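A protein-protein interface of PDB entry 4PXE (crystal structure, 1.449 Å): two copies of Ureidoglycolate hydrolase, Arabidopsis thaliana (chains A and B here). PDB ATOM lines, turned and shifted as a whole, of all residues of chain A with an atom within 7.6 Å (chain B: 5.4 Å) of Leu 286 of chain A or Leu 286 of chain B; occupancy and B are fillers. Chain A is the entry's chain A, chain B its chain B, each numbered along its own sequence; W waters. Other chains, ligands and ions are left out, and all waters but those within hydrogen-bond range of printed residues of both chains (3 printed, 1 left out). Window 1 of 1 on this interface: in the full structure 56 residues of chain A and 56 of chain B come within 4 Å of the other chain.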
ATOM      1  N   ALA A 256      -5.517  11.748 -18.618  1.00  0.00           N
ATOM      2  CA  ALA A 256      -4.521  11.151 -19.507  1.00  0.00           C
ATOM      3  C   ALA A 256      -4.189  12.061 -20.681  1.00  0.00           C
ATOM      4  O   ALA A 256      -3.108  11.962 -21.260  1.00  0.00           O
ATOM      5  CB  ALA A 256      -4.995   9.790 -20.004  1.00  0.00           C
ATOM      6  N   GLY A 257      -5.120  12.936 -21.041  1.00  0.00           N
ATOM      7  CA  GLY A 257      -4.883  13.864 -22.134  1.00  0.00           C
ATOM      8  C   GLY A 257      -3.851  14.905 -21.744  1.00  0.00           C
ATOM      9  O   GLY A 257      -2.990  15.271 -22.554  1.00  0.00           O
ATOM     10  N   LEU A 258      -3.914  15.380 -20.508  1.00  0.00           N
ATOM     11  CA  LEU A 258      -2.949  16.363 -20.035  1.00  0.00           C
ATOM     12  C   LEU A 258      -1.568  15.735 -19.860  1.00  0.00           C
ATOM     13  O   LEU A 258      -0.563  16.391 -20.149  1.00  0.00           O
ATOM     14  CB  LEU A 258      -3.444  17.047 -18.768  1.00  0.00           C
ATOM     15  CG  LEU A 258      -4.679  17.912 -19.003  1.00  0.00           C
ATOM     16  CD1 LEU A 258      -5.098  18.593 -17.718  1.00  0.00           C
ATOM     17  CD2 LEU A 258      -4.429  18.948 -20.114  1.00  0.00           C
ATOM     18  N   ALA A 259      -1.510  14.467 -19.451  1.00  0.00           N
ATOM     19  CA  ALA A 259      -0.233  13.754 -19.432  1.00  0.00           C
ATOM     20  C   ALA A 259       0.370  13.708 -20.829  1.00  0.00           C
ATOM     21  O   ALA A 259       1.572  13.923 -21.003  1.00  0.00           O
ATOM     22  CB  ALA A 259      -0.400  12.344 -18.880  1.00  0.00           C
ATOM     23  N   ALA A 260      -0.462  13.442 -21.830  1.00  0.00           N
ATOM     24  CA  ALA A 260       0.003  13.362 -23.209  1.00  0.00           C
ATOM     25  C   ALA A 260       0.491  14.717 -23.694  1.00  0.00           C
ATOM     26  O   ALA A 260       1.529  14.806 -24.365  1.00  0.00           O
ATOM     27  CB  ALA A 260      -1.103  12.837 -24.107  1.00  0.00           C
ATOM     28  N   ALA A 261      -0.243  15.772 -23.352  1.00  0.00           N
ATOM     29  CA  ALA A 261       0.150  17.129 -23.741  1.00  0.00           C
ATOM     30  C   ALA A 261       1.515  17.483 -23.156  1.00  0.00           C
ATOM     31  O   ALA A 261       2.387  18.037 -23.850  1.00  0.00           O
ATOM     32  CB  ALA A 261      -0.901  18.132 -23.291  1.00  0.00           C
ATOM     33  N   GLU A 262       1.711  17.138 -21.890  1.00  0.00           N
ATOM     34  CA  GLU A 262       2.980  17.400 -21.226  1.00  0.00           C
ATOM     35  C   GLU A 262       4.110  16.603 -21.849  1.00  0.00           C
ATOM     36  O   GLU A 262       5.228  17.120 -21.991  1.00  0.00           O
ATOM     37  CB  GLU A 262       2.873  17.125 -19.722  1.00  0.00           C
ATOM     38  CG  GLU A 262       1.996  18.149 -19.043  1.00  0.00           C
ATOM     39  CD  GLU A 262       1.671  17.838 -17.594  1.00  0.00           C
ATOM     40  OE1 GLU A 262       1.539  16.647 -17.243  1.00  0.00           O
ATOM     41  OE2 GLU A 262       1.528  18.803 -16.816  1.00  0.00           O
ATOM     42  N   LEU A 263       3.839  15.357 -22.236  1.00  0.00           N
ATOM     43  CA  LEU A 263       4.888  14.548 -22.854  1.00  0.00           C
ATOM     44  C   LEU A 263       5.267  15.102 -24.219  1.00  0.00           C
ATOM     45  O   LEU A 263       6.449  15.142 -24.552  1.00  0.00           O
ATOM     46  CB  LEU A 263       4.514  13.064 -22.943  1.00  0.00           C
ATOM     47  CG  LEU A 263       5.644  12.138 -23.422  1.00  0.00           C
ATOM     48  CD1 LEU A 263       6.906  12.242 -22.540  1.00  0.00           C
ATOM     49  CD2 LEU A 263       5.177  10.702 -23.527  1.00  0.00           C
ATOM     50  N   ALA A 264       4.287  15.550 -24.997  1.00  0.00           N
ATOM     51  CA  ALA A 264       4.598  16.107 -26.320  1.00  0.00           C
ATOM     52  C   ALA A 264       5.499  17.323 -26.184  1.00  0.00           C
ATOM     53  O   ALA A 264       6.436  17.495 -26.976  1.00  0.00           O
ATOM     54  CB  ALA A 264       3.316  16.472 -27.058  1.00  0.00           C
ATOM     55  N   LEU A 265       5.228  18.171 -25.196  1.00  0.00           N
ATOM     56  CA  LEU A 265       6.054  19.349 -24.960  1.00  0.00           C
ATOM     57  C   LEU A 265       7.440  18.952 -24.436  1.00  0.00           C
ATOM     58  O   LEU A 265       8.442  19.617 -24.744  1.00  0.00           O
ATOM     59  CB  LEU A 265       5.347  20.332 -24.020  1.00  0.00           C
ATOM     60  CG  LEU A 265       4.157  21.005 -24.716  1.00  0.00           C
ATOM     61  CD1 LEU A 265       3.133  21.542 -23.719  1.00  0.00           C
ATOM     62  CD2 LEU A 265       4.627  22.115 -25.647  1.00  0.00           C
ATOM     63  N   VAL A 283       5.703  14.674 -32.305  1.00  0.00           N
ATOM     64  CA  VAL A 283       4.534  13.879 -31.971  1.00  0.00           C
ATOM     65  C   VAL A 283       3.504  14.070 -33.085  1.00  0.00           C
ATOM     66  O   VAL A 283       2.786  15.063 -33.118  1.00  0.00           O
ATOM     67  CB  VAL A 283       3.951  14.295 -30.612  1.00  0.00           C
ATOM     68  CG1 VAL A 283       2.691  13.484 -30.299  1.00  0.00           C
ATOM     69  CG2 VAL A 283       5.009  14.129 -29.509  1.00  0.00           C
ATOM     70  N   GLY A 284       3.460  13.114 -34.012  1.00  0.00           N
ATOM     71  CA  GLY A 284       2.550  13.198 -35.142  1.00  0.00           C
ATOM     72  C   GLY A 284       1.199  12.568 -34.863  1.00  0.00           C
ATOM     73  O   GLY A 284       0.228  12.851 -35.556  1.00  0.00           O
ATOM     74  N   ILE A 285       1.150  11.704 -33.852  1.00  0.00           N
ATOM     75  CA  ILE A 285      -0.090  11.049 -33.454  1.00  0.00           C
ATOM     76  C   ILE A 285      -0.326  11.259 -31.961  1.00  0.00           C
ATOM     77  O   ILE A 285       0.565  11.019 -31.141  1.00  0.00           O
ATOM     78  CB  ILE A 285      -0.057   9.542 -33.782  1.00  0.00           C
ATOM     79  CG1 ILE A 285      -0.155   9.331 -35.295  1.00  0.00           C
ATOM     80  CG2 ILE A 285      -1.175   8.791 -33.038  1.00  0.00           C
ATOM     81  CD1 ILE A 285       0.085   7.895 -35.735  1.00  0.00           C
ATOM     82  N   LEU A 286      -1.520  11.741 -31.624  1.00  0.00           N
ATOM     83  CA  LEU A 286      -1.923  11.910 -30.231  1.00  0.00           C
ATOM     84  C   LEU A 286      -3.420  11.659 -30.226  1.00  0.00           C
ATOM     85  O   LEU A 286      -4.183  12.476 -30.751  1.00  0.00           O
ATOM     86  CB  LEU A 286      -1.589  13.323 -29.724  1.00  0.00           C
ATOM     87  CG  LEU A 286      -1.573  13.552 -28.204  1.00  0.00           C
ATOM     88  CD1 LEU A 286      -1.027  14.934 -27.843  1.00  0.00           C
ATOM     89  CD2 LEU A 286      -2.962  13.376 -27.587  1.00  0.00           C
ATOM     90  N   GLU A 287      -3.829  10.530 -29.647  1.00  0.00           N
ATOM     91  CA  GLU A 287      -5.233  10.135 -29.658  1.00  0.00           C
ATOM     92  C   GLU A 287      -5.768  10.011 -28.250  1.00  0.00           C
ATOM     93  O   GLU A 287      -5.096   9.469 -27.365  1.00  0.00           O
ATOM     94  CB  GLU A 287      -5.408   8.813 -30.399  1.00  0.00           C
ATOM     95  CG  GLU A 287      -4.972   8.886 -31.860  1.00  0.00           C
ATOM     96  CD  GLU A 287      -5.033   7.549 -32.567  1.00  0.00           C
ATOM     97  OE1 GLU A 287      -4.996   6.506 -31.881  1.00  0.00           O
ATOM     98  OE2 GLU A 287      -5.108   7.546 -33.817  1.00  0.00           O
ATOM     99  N   LEU A 288      -6.977  10.526 -28.052  1.00  0.00           N
ATOM    100  CA  LEU A 288      -7.655  10.436 -26.759  1.00  0.00           C
ATOM    101  C   LEU A 288      -8.807   9.441 -26.801  1.00  0.00           C
ATOM    102  O   LEU A 288      -9.528   9.334 -27.794  1.00  0.00           O
ATOM    103  CB  LEU A 288      -8.180  11.801 -26.331  1.00  0.00           C
ATOM    104  CG  LEU A 288      -7.200  12.976 -26.300  1.00  0.00           C
ATOM    105  CD1 LEU A 288      -7.897  14.269 -25.881  1.00  0.00           C
ATOM    106  CD2 LEU A 288      -6.007  12.647 -25.386  1.00  0.00           C
ATOM    107  N   GLY A 291     -12.674  10.098 -26.293  1.00  0.00           N
ATOM    108  CA  GLY A 291     -12.780  11.100 -27.342  1.00  0.00           C
ATOM    109  C   GLY A 291     -14.166  11.702 -27.455  1.00  0.00           C
ATOM    110  O   GLY A 291     -14.720  11.821 -28.552  1.00  0.00           O
ATOM    111  N   ALA A 292     -14.733  12.069 -26.314  1.00  0.00           N
ATOM    112  CA  ALA A 292     -16.010  12.768 -26.292  1.00  0.00           C
ATOM    113  C   ALA A 292     -15.809  14.061 -25.520  1.00  0.00           C
ATOM    114  O   ALA A 292     -15.021  14.106 -24.576  1.00  0.00           O
ATOM    115  CB  ALA A 292     -17.075  11.915 -25.635  1.00  0.00           C
ATOM    116  N   PRO A 297     -10.536  12.225 -20.671  1.00  0.00           N
ATOM    117  CA  PRO A 297      -9.798  11.110 -21.280  1.00  0.00           C
ATOM    118  C   PRO A 297      -9.239  10.128 -20.250  1.00  0.00           C
ATOM    119  O   PRO A 297      -8.540  10.544 -19.324  1.00  0.00           O
ATOM    120  CB  PRO A 297      -8.651  11.810 -22.023  1.00  0.00           C
ATOM    121  CG  PRO A 297      -9.188  13.170 -22.345  1.00  0.00           C
ATOM    122  CD  PRO A 297     -10.078  13.539 -21.163  1.00  0.00           C
ATOM    123  N   LYS A 299      -7.638   7.272 -21.480  1.00  0.00           N
ATOM    124  CA  LYS A 299      -6.467   6.731 -22.154  1.00  0.00           C
ATOM    125  C   LYS A 299      -5.973   7.740 -23.171  1.00  0.00           C
ATOM    126  O   LYS A 299      -6.763   8.385 -23.852  1.00  0.00           O
ATOM    127  CB  LYS A 299      -6.791   5.417 -22.855  1.00  0.00           C
ATOM    128  CG  LYS A 299      -7.105   4.254 -21.941  1.00  0.00           C
ATOM    129  CD  LYS A 299      -6.912   2.932 -22.666  1.00  0.00           C
ATOM    130  CE  LYS A 299      -7.650   2.905 -23.997  1.00  0.00           C
ATOM    131  NZ  LYS A 299      -7.462   1.600 -24.699  1.00  0.00           N
ATOM    132  N   SER A 300      -4.658   7.892 -23.258  1.00  0.00           N
ATOM    133  CA  SER A 300      -4.074   8.664 -24.342  1.00  0.00           C
ATOM    134  C   SER A 300      -2.976   7.839 -24.986  1.00  0.00           C
ATOM    135  O   SER A 300      -2.350   7.005 -24.339  1.00  0.00           O
ATOM    136  CB  SER A 300      -3.538  10.001 -23.843  1.00  0.00           C
ATOM    137  OG  SER A 300      -2.514   9.822 -22.876  1.00  0.00           O
ATOM    138  N   HIS A 301      -2.759   8.080 -26.273  1.00  0.00           N
ATOM    139  CA  HIS A 301      -1.867   7.278 -27.095  1.00  0.00           C
ATOM    140  C   HIS A 301      -1.054   8.246 -27.934  1.00  0.00           C
ATOM    141  O   HIS A 301      -1.626   9.021 -28.709  1.00  0.00           O
ATOM    142  CB  HIS A 301      -2.716   6.363 -27.995  1.00  0.00           C
ATOM    143  CG  HIS A 301      -1.935   5.610 -29.029  1.00  0.00           C
ATOM    144  ND1 HIS A 301      -1.492   4.317 -28.837  1.00  0.00           N
ATOM    145  CD2 HIS A 301      -1.545   5.960 -30.277  1.00  0.00           C
ATOM    146  CE1 HIS A 301      -0.844   3.912 -29.918  1.00  0.00           C
ATOM    147  NE2 HIS A 301      -0.864   4.889 -30.806  1.00  0.00           N
ATOM    148  N   LEU A 302       0.267   8.219 -27.762  1.00  0.00           N
ATOM    149  CA  LEU A 302       1.175   9.062 -28.545  1.00  0.00           C
ATOM    150  C   LEU A 302       2.095   8.198 -29.369  1.00  0.00           C
ATOM    151  O   LEU A 302       2.535   7.140 -28.918  1.00  0.00           O
ATOM    152  CB  LEU A 302       2.083   9.904 -27.652  1.00  0.00           C
ATOM    153  CG  LEU A 302       1.484  10.835 -26.619  1.00  0.00           C
ATOM    154  CD1 LEU A 302       1.275  10.053 -25.333  1.00  0.00           C
ATOM    155  CD2 LEU A 302       2.385  12.048 -26.399  1.00  0.00           C
ATOM    156  N   GLU A 303       2.415   8.662 -30.571  1.00  0.00           N
ATOM    157  CA  GLU A 303       3.475   8.041 -31.349  1.00  0.00           C
ATOM    158  C   GLU A 303       4.481   9.125 -31.685  1.00  0.00           C
ATOM    159  O   GLU A 303       4.127  10.187 -32.216  1.00  0.00           O
ATOM    160  CB  GLU A 303       2.921   7.341 -32.592  1.00  0.00           C
ATOM    161  CG  GLU A 303       1.842   6.349 -32.218  1.00  0.00           C
ATOM    162  CD  GLU A 303       1.412   5.445 -33.352  1.00  0.00           C
ATOM    163  OE1 GLU A 303       2.173   5.278 -34.330  1.00  0.00           O
ATOM    164  OE2 GLU A 303       0.301   4.888 -33.255  1.00  0.00           O
ATOM    165  N   ALA B 260      -1.926  22.902 -29.677  1.00  0.00           N
ATOM    166  CA  ALA B 260      -3.064  22.253 -29.021  1.00  0.00           C
ATOM    167  C   ALA B 260      -2.689  21.775 -27.623  1.00  0.00           C
ATOM    168  O   ALA B 260      -3.450  21.981 -26.680  1.00  0.00           O
ATOM    169  CB  ALA B 260      -3.590  21.096 -29.861  1.00  0.00           C
ATOM    170  N   ALA B 261      -1.510  21.178 -27.474  1.00  0.00           N
ATOM    171  CA  ALA B 261      -1.043  20.730 -26.164  1.00  0.00           C
ATOM    172  C   ALA B 261      -0.967  21.894 -25.182  1.00  0.00           C
ATOM    173  O   ALA B 261      -1.425  21.793 -24.026  1.00  0.00           O
ATOM    174  CB  ALA B 261       0.321  20.046 -26.288  1.00  0.00           C
ATOM    175  N   ALA B 264      -4.500  23.018 -24.176  1.00  0.00           N
ATOM    176  CA  ALA B 264      -5.126  22.088 -23.229  1.00  0.00           C
ATOM    177  C   ALA B 264      -4.627  22.350 -21.811  1.00  0.00           C
ATOM    178  O   ALA B 264      -5.417  22.377 -20.851  1.00  0.00           O
ATOM    179  CB  ALA B 264      -4.883  20.652 -23.630  1.00  0.00           C
ATOM    180  N   VAL B 283     -10.545  19.135 -21.801  1.00  0.00           N
ATOM    181  CA  VAL B 283     -10.361  18.896 -23.228  1.00  0.00           C
ATOM    182  C   VAL B 283     -10.599  17.410 -23.475  1.00  0.00           C
ATOM    183  O   VAL B 283      -9.728  16.574 -23.205  1.00  0.00           O
ATOM    184  CB  VAL B 283      -8.952  19.282 -23.725  1.00  0.00           C
ATOM    185  CG1 VAL B 283      -8.803  18.914 -25.207  1.00  0.00           C
ATOM    186  CG2 VAL B 283      -8.690  20.768 -23.495  1.00  0.00           C
ATOM    187  N   GLY B 284     -11.799  17.076 -23.942  1.00  0.00           N
ATOM    188  CA  GLY B 284     -12.130  15.687 -24.185  1.00  0.00           C
ATOM    189  C   GLY B 284     -11.875  15.228 -25.603  1.00  0.00           C
ATOM    190  O   GLY B 284     -11.840  14.035 -25.875  1.00  0.00           O
ATOM    191  N   ILE B 285     -11.713  16.184 -26.515  1.00  0.00           N
ATOM    192  CA  ILE B 285     -11.418  15.868 -27.909  1.00  0.00           C
ATOM    193  C   ILE B 285     -10.205  16.679 -28.316  1.00  0.00           C
ATOM    194  O   ILE B 285     -10.165  17.893 -28.109  1.00  0.00           O
ATOM    195  CB  ILE B 285     -12.621  16.210 -28.806  1.00  0.00           C
ATOM    196  CG1 ILE B 285     -13.755  15.208 -28.557  1.00  0.00           C
ATOM    197  CG2 ILE B 285     -12.216  16.197 -30.287  1.00  0.00           C
ATOM    198  CD1 ILE B 285     -15.063  15.571 -29.237  1.00  0.00           C
ATOM    199  N   LEU B 286      -9.204  15.996 -28.860  1.00  0.00           N
ATOM    200  CA  LEU B 286      -8.012  16.655 -29.391  1.00  0.00           C
ATOM    201  C   LEU B 286      -7.569  15.794 -30.549  1.00  0.00           C
ATOM    202  O   LEU B 286      -7.073  14.680 -30.338  1.00  0.00           O
ATOM    203  CB  LEU B 286      -6.909  16.757 -28.328  1.00  0.00           C
ATOM    204  CG  LEU B 286      -5.744  17.732 -28.573  1.00  0.00           C
ATOM    205  CD1 LEU B 286      -4.919  17.899 -27.314  1.00  0.00           C
ATOM    206  CD2 LEU B 286      -4.846  17.263 -29.720  1.00  0.00           C
ATOM    207  N   GLU B 287      -7.760  16.304 -31.764  1.00  0.00           N
ATOM    208  CA  GLU B 287      -7.459  15.571 -32.991  1.00  0.00           C
ATOM    209  C   GLU B 287      -6.379  16.262 -33.816  1.00  0.00           C
ATOM    210  O   GLU B 287      -6.406  17.478 -34.003  1.00  0.00           O
ATOM    211  CB  GLU B 287      -8.726  15.419 -33.831  1.00  0.00           C
ATOM    212  CG  GLU B 287      -9.790  14.585 -33.146  1.00  0.00           C
ATOM    213  CD  GLU B 287     -11.125  14.623 -33.861  1.00  0.00           C
ATOM    214  OE1 GLU B 287     -11.260  15.389 -34.840  1.00  0.00           O
ATOM    215  OE2 GLU B 287     -12.041  13.886 -33.436  1.00  0.00           O
ATOM    216  N   LEU B 288      -5.425  15.472 -34.303  1.00  0.00           N
ATOM    217  CA  LEU B 288      -4.351  15.989 -35.138  1.00  0.00           C
ATOM    218  C   LEU B 288      -4.530  15.567 -36.588  1.00  0.00           C
ATOM    219  O   LEU B 288      -4.988  14.463 -36.887  1.00  0.00           O
ATOM    220  CB  LEU B 288      -3.001  15.474 -34.652  1.00  0.00           C
ATOM    221  CG  LEU B 288      -2.655  15.755 -33.192  1.00  0.00           C
ATOM    222  CD1 LEU B 288      -1.264  15.231 -32.896  1.00  0.00           C
ATOM    223  CD2 LEU B 288      -2.742  17.242 -32.893  1.00  0.00           C
ATOM    224  N   SER B 300      -4.779  21.181 -35.879  1.00  0.00           N
ATOM    225  CA  SER B 300      -5.229  20.528 -34.657  1.00  0.00           C
ATOM    226  C   SER B 300      -6.623  21.036 -34.337  1.00  0.00           C
ATOM    227  O   SER B 300      -6.966  22.175 -34.659  1.00  0.00           O
ATOM    228  CB  SER B 300      -4.258  20.753 -33.499  1.00  0.00           C
ATOM    229  OG  SER B 300      -4.103  22.128 -33.208  1.00  0.00           O
ATOM    230  N   HIS B 301      -7.424  20.178 -33.720  1.00  0.00           N
ATOM    231  CA  HIS B 301      -8.821  20.482 -33.409  1.00  0.00           C
ATOM    232  C   HIS B 301      -9.086  20.067 -31.969  1.00  0.00           C
ATOM    233  O   HIS B 301      -8.902  18.897 -31.624  1.00  0.00           O
ATOM    234  CB  HIS B 301      -9.712  19.678 -34.366  1.00  0.00           C
ATOM    235  CG  HIS B 301     -11.182  19.746 -34.064  1.00  0.00           C
ATOM    236  ND1 HIS B 301     -12.035  20.605 -34.721  1.00  0.00           N
ATOM    237  CD2 HIS B 301     -11.956  19.026 -33.215  1.00  0.00           C
ATOM    238  CE1 HIS B 301     -13.264  20.442 -34.261  1.00  0.00           C
ATOM    239  NE2 HIS B 301     -13.243  19.490 -33.346  1.00  0.00           N
ATOM    240  N   LEU B 302      -9.510  21.020 -31.135  1.00  0.00           N
ATOM    241  CA  LEU B 302      -9.856  20.760 -29.728  1.00  0.00           C
ATOM    242  C   LEU B 302     -11.314  21.071 -29.482  1.00  0.00           C
ATOM    243  O   LEU B 302     -11.848  22.035 -30.027  1.00  0.00           O
ATOM    244  CB  LEU B 302      -9.061  21.660 -28.774  1.00  0.00           C
ATOM    245  CG  LEU B 302      -7.538  21.674 -28.826  1.00  0.00           C
ATOM    246  CD1 LEU B 302      -7.066  22.704 -29.861  1.00  0.00           C
ATOM    247  CD2 LEU B 302      -6.955  21.963 -27.453  1.00  0.00           C
ATOM    248  N   GLU B 303     -11.954  20.271 -28.635  1.00  0.00           N
ATOM    249  CA  GLU B 303     -13.283  20.626 -28.140  1.00  0.00           C
ATOM    250  C   GLU B 303     -13.222  20.640 -26.632  1.00  0.00           C
ATOM    251  O   GLU B 303     -12.728  19.694 -26.004  1.00  0.00           O
ATOM    252  CB  GLU B 303     -14.366  19.684 -28.677  1.00  0.00           C
ATOM    253  CG  GLU B 303     -14.301  19.593 -30.195  1.00  0.00           C
ATOM    254  CD  GLU B 303     -15.502  18.941 -30.847  1.00  0.00           C
ATOM    255  OE1 GLU B 303     -16.559  18.808 -30.196  1.00  0.00           O
ATOM    256  OE2 GLU B 303     -15.386  18.567 -32.031  1.00  0.00           O
HETATM  257  O   HOH W   1     -12.478  12.036 -24.123  1.00  0.00           O
HETATM  258  O   HOH W   2      -5.632  12.840 -33.123  1.00  0.00           O
HETATM  259  O   HOH W   3      -7.894  11.981 -30.341  1.00  0.00           O
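O of Pro 297 of chain A lies within hydrogen-bond range of N of Ala 256 of chain A. O of Ile 285 of chain B lies within hydrogen-bond range of N of Glu 303 of chain B (3.0 Å). N of Gly 284 of chain B sits at hydrogen-bond distance from O of Glu 303 of chain B. The backbone carbonyl oxygen (O) of Glu 303 of chain A lies within hydrogen-bond range of the backbone NH (N) of Gly 284 of chain A.
Ala 261 of chain B touches its own counterpart, Ala 261 of chain A. Gly 284 of chain A touches Leu 288 of chain B, and with the chains exchanged Leu 288 of chain A touches Gly 284 of chain B. Leu 286 of chain A touches Leu 288 of chain B, and with the chains exchanged Leu 288 of chain A touches Leu 286 of chain B. Leu 288 of chain A touches Val 283 of chain B, but with the chains exchanged Val 283 of chain A does not touch Leu 288 of chain B (4.1 Å).
Among the printed residues, pairs that only touch across the chains: Gly 291 of chain A with Gly 284 of chain B (3.4 Å), Gly 291 of chain A with Ile 285 of chain B (3.5 Å), Pro 297 of chain A with Val 283 of chain B (3.6 Å), Leu 288 of chain A with Leu 286 of chain B (3.6 Å), Leu 258 of chain A with Ala 264 of chain B (3.6 Å), Leu 286 of chain A with Leu 286 of chain B (3.7 Å), Leu 286 of chain A with Leu 288 of chain B (3.7 Å), Ala 261 of chain A with Ala 261 of chain B (3.8 Å), Ala 292 of chain A with Ile 285 of chain B (3.8 Å), Gly 284 of chain A with Leu 288 of chain B (3.9 Å), Leu 288 of chain A with Gly 284 of chain B (3.9 Å) and Leu 288 of chain A with Val 283 of chain B (3.98 Å).
The backbone carbonyl oxygen (O) of Gly 284 of chain B lies close to the backbone carbonyl oxygen (O) of Ala 292 of chain A (3.4 Å).
Water W1 lies within hydrogen-bond range of O of Gly 284 of chain B, N of Gly 291 of chain A and N of Ala 292 of chain A. Water W2 lies within hydrogen-bond range of O of Leu 286 of chain A and N of Leu 288 of chain B. Water W3 bridges the backbone carbonyl oxygen (O) of Leu 286 of chain B (2.8 Å) and the backbone NH (N) of Leu 288 of chain A (2.9 Å).
Leu 286 of chain A touches two residues of chain B. Leu 286 of chain B touches two residues of chain A. Of the printed residues of chain A, Ile 285 of chain B touches Gly 291 (3.5 Å) and Ala 292 (3.8 Å). Of the printed residues of chain B, Pro 297 of chain A touches Val 283. Of the printed residues of chain B, Gly 291 of chain A touches Gly 284 (3.4 Å) and Ile 285 (3.5 Å). The nearest residue of chain A that does not touch Leu 286 of chain B is Glu 287 of chain A (5.0 Å).
Of the 24 printed residues of chain A, 8 touch a printed residue of chain B. Printed residues of chain A that touch a printed residue of chain B: Leu 258, Ala 261, Gly 284, Leu 286, Leu 288, Gly 291, Ala 292 and Pro 297. Hydrophobic or aromatic side chains of chain A within 4 Å of the printed part of chain B: Leu 258, Ala 261, Leu 286, Leu 288 and Pro 297. Along chain A the printed residues that touch a printed residue of chain B span positions 258 to 297.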
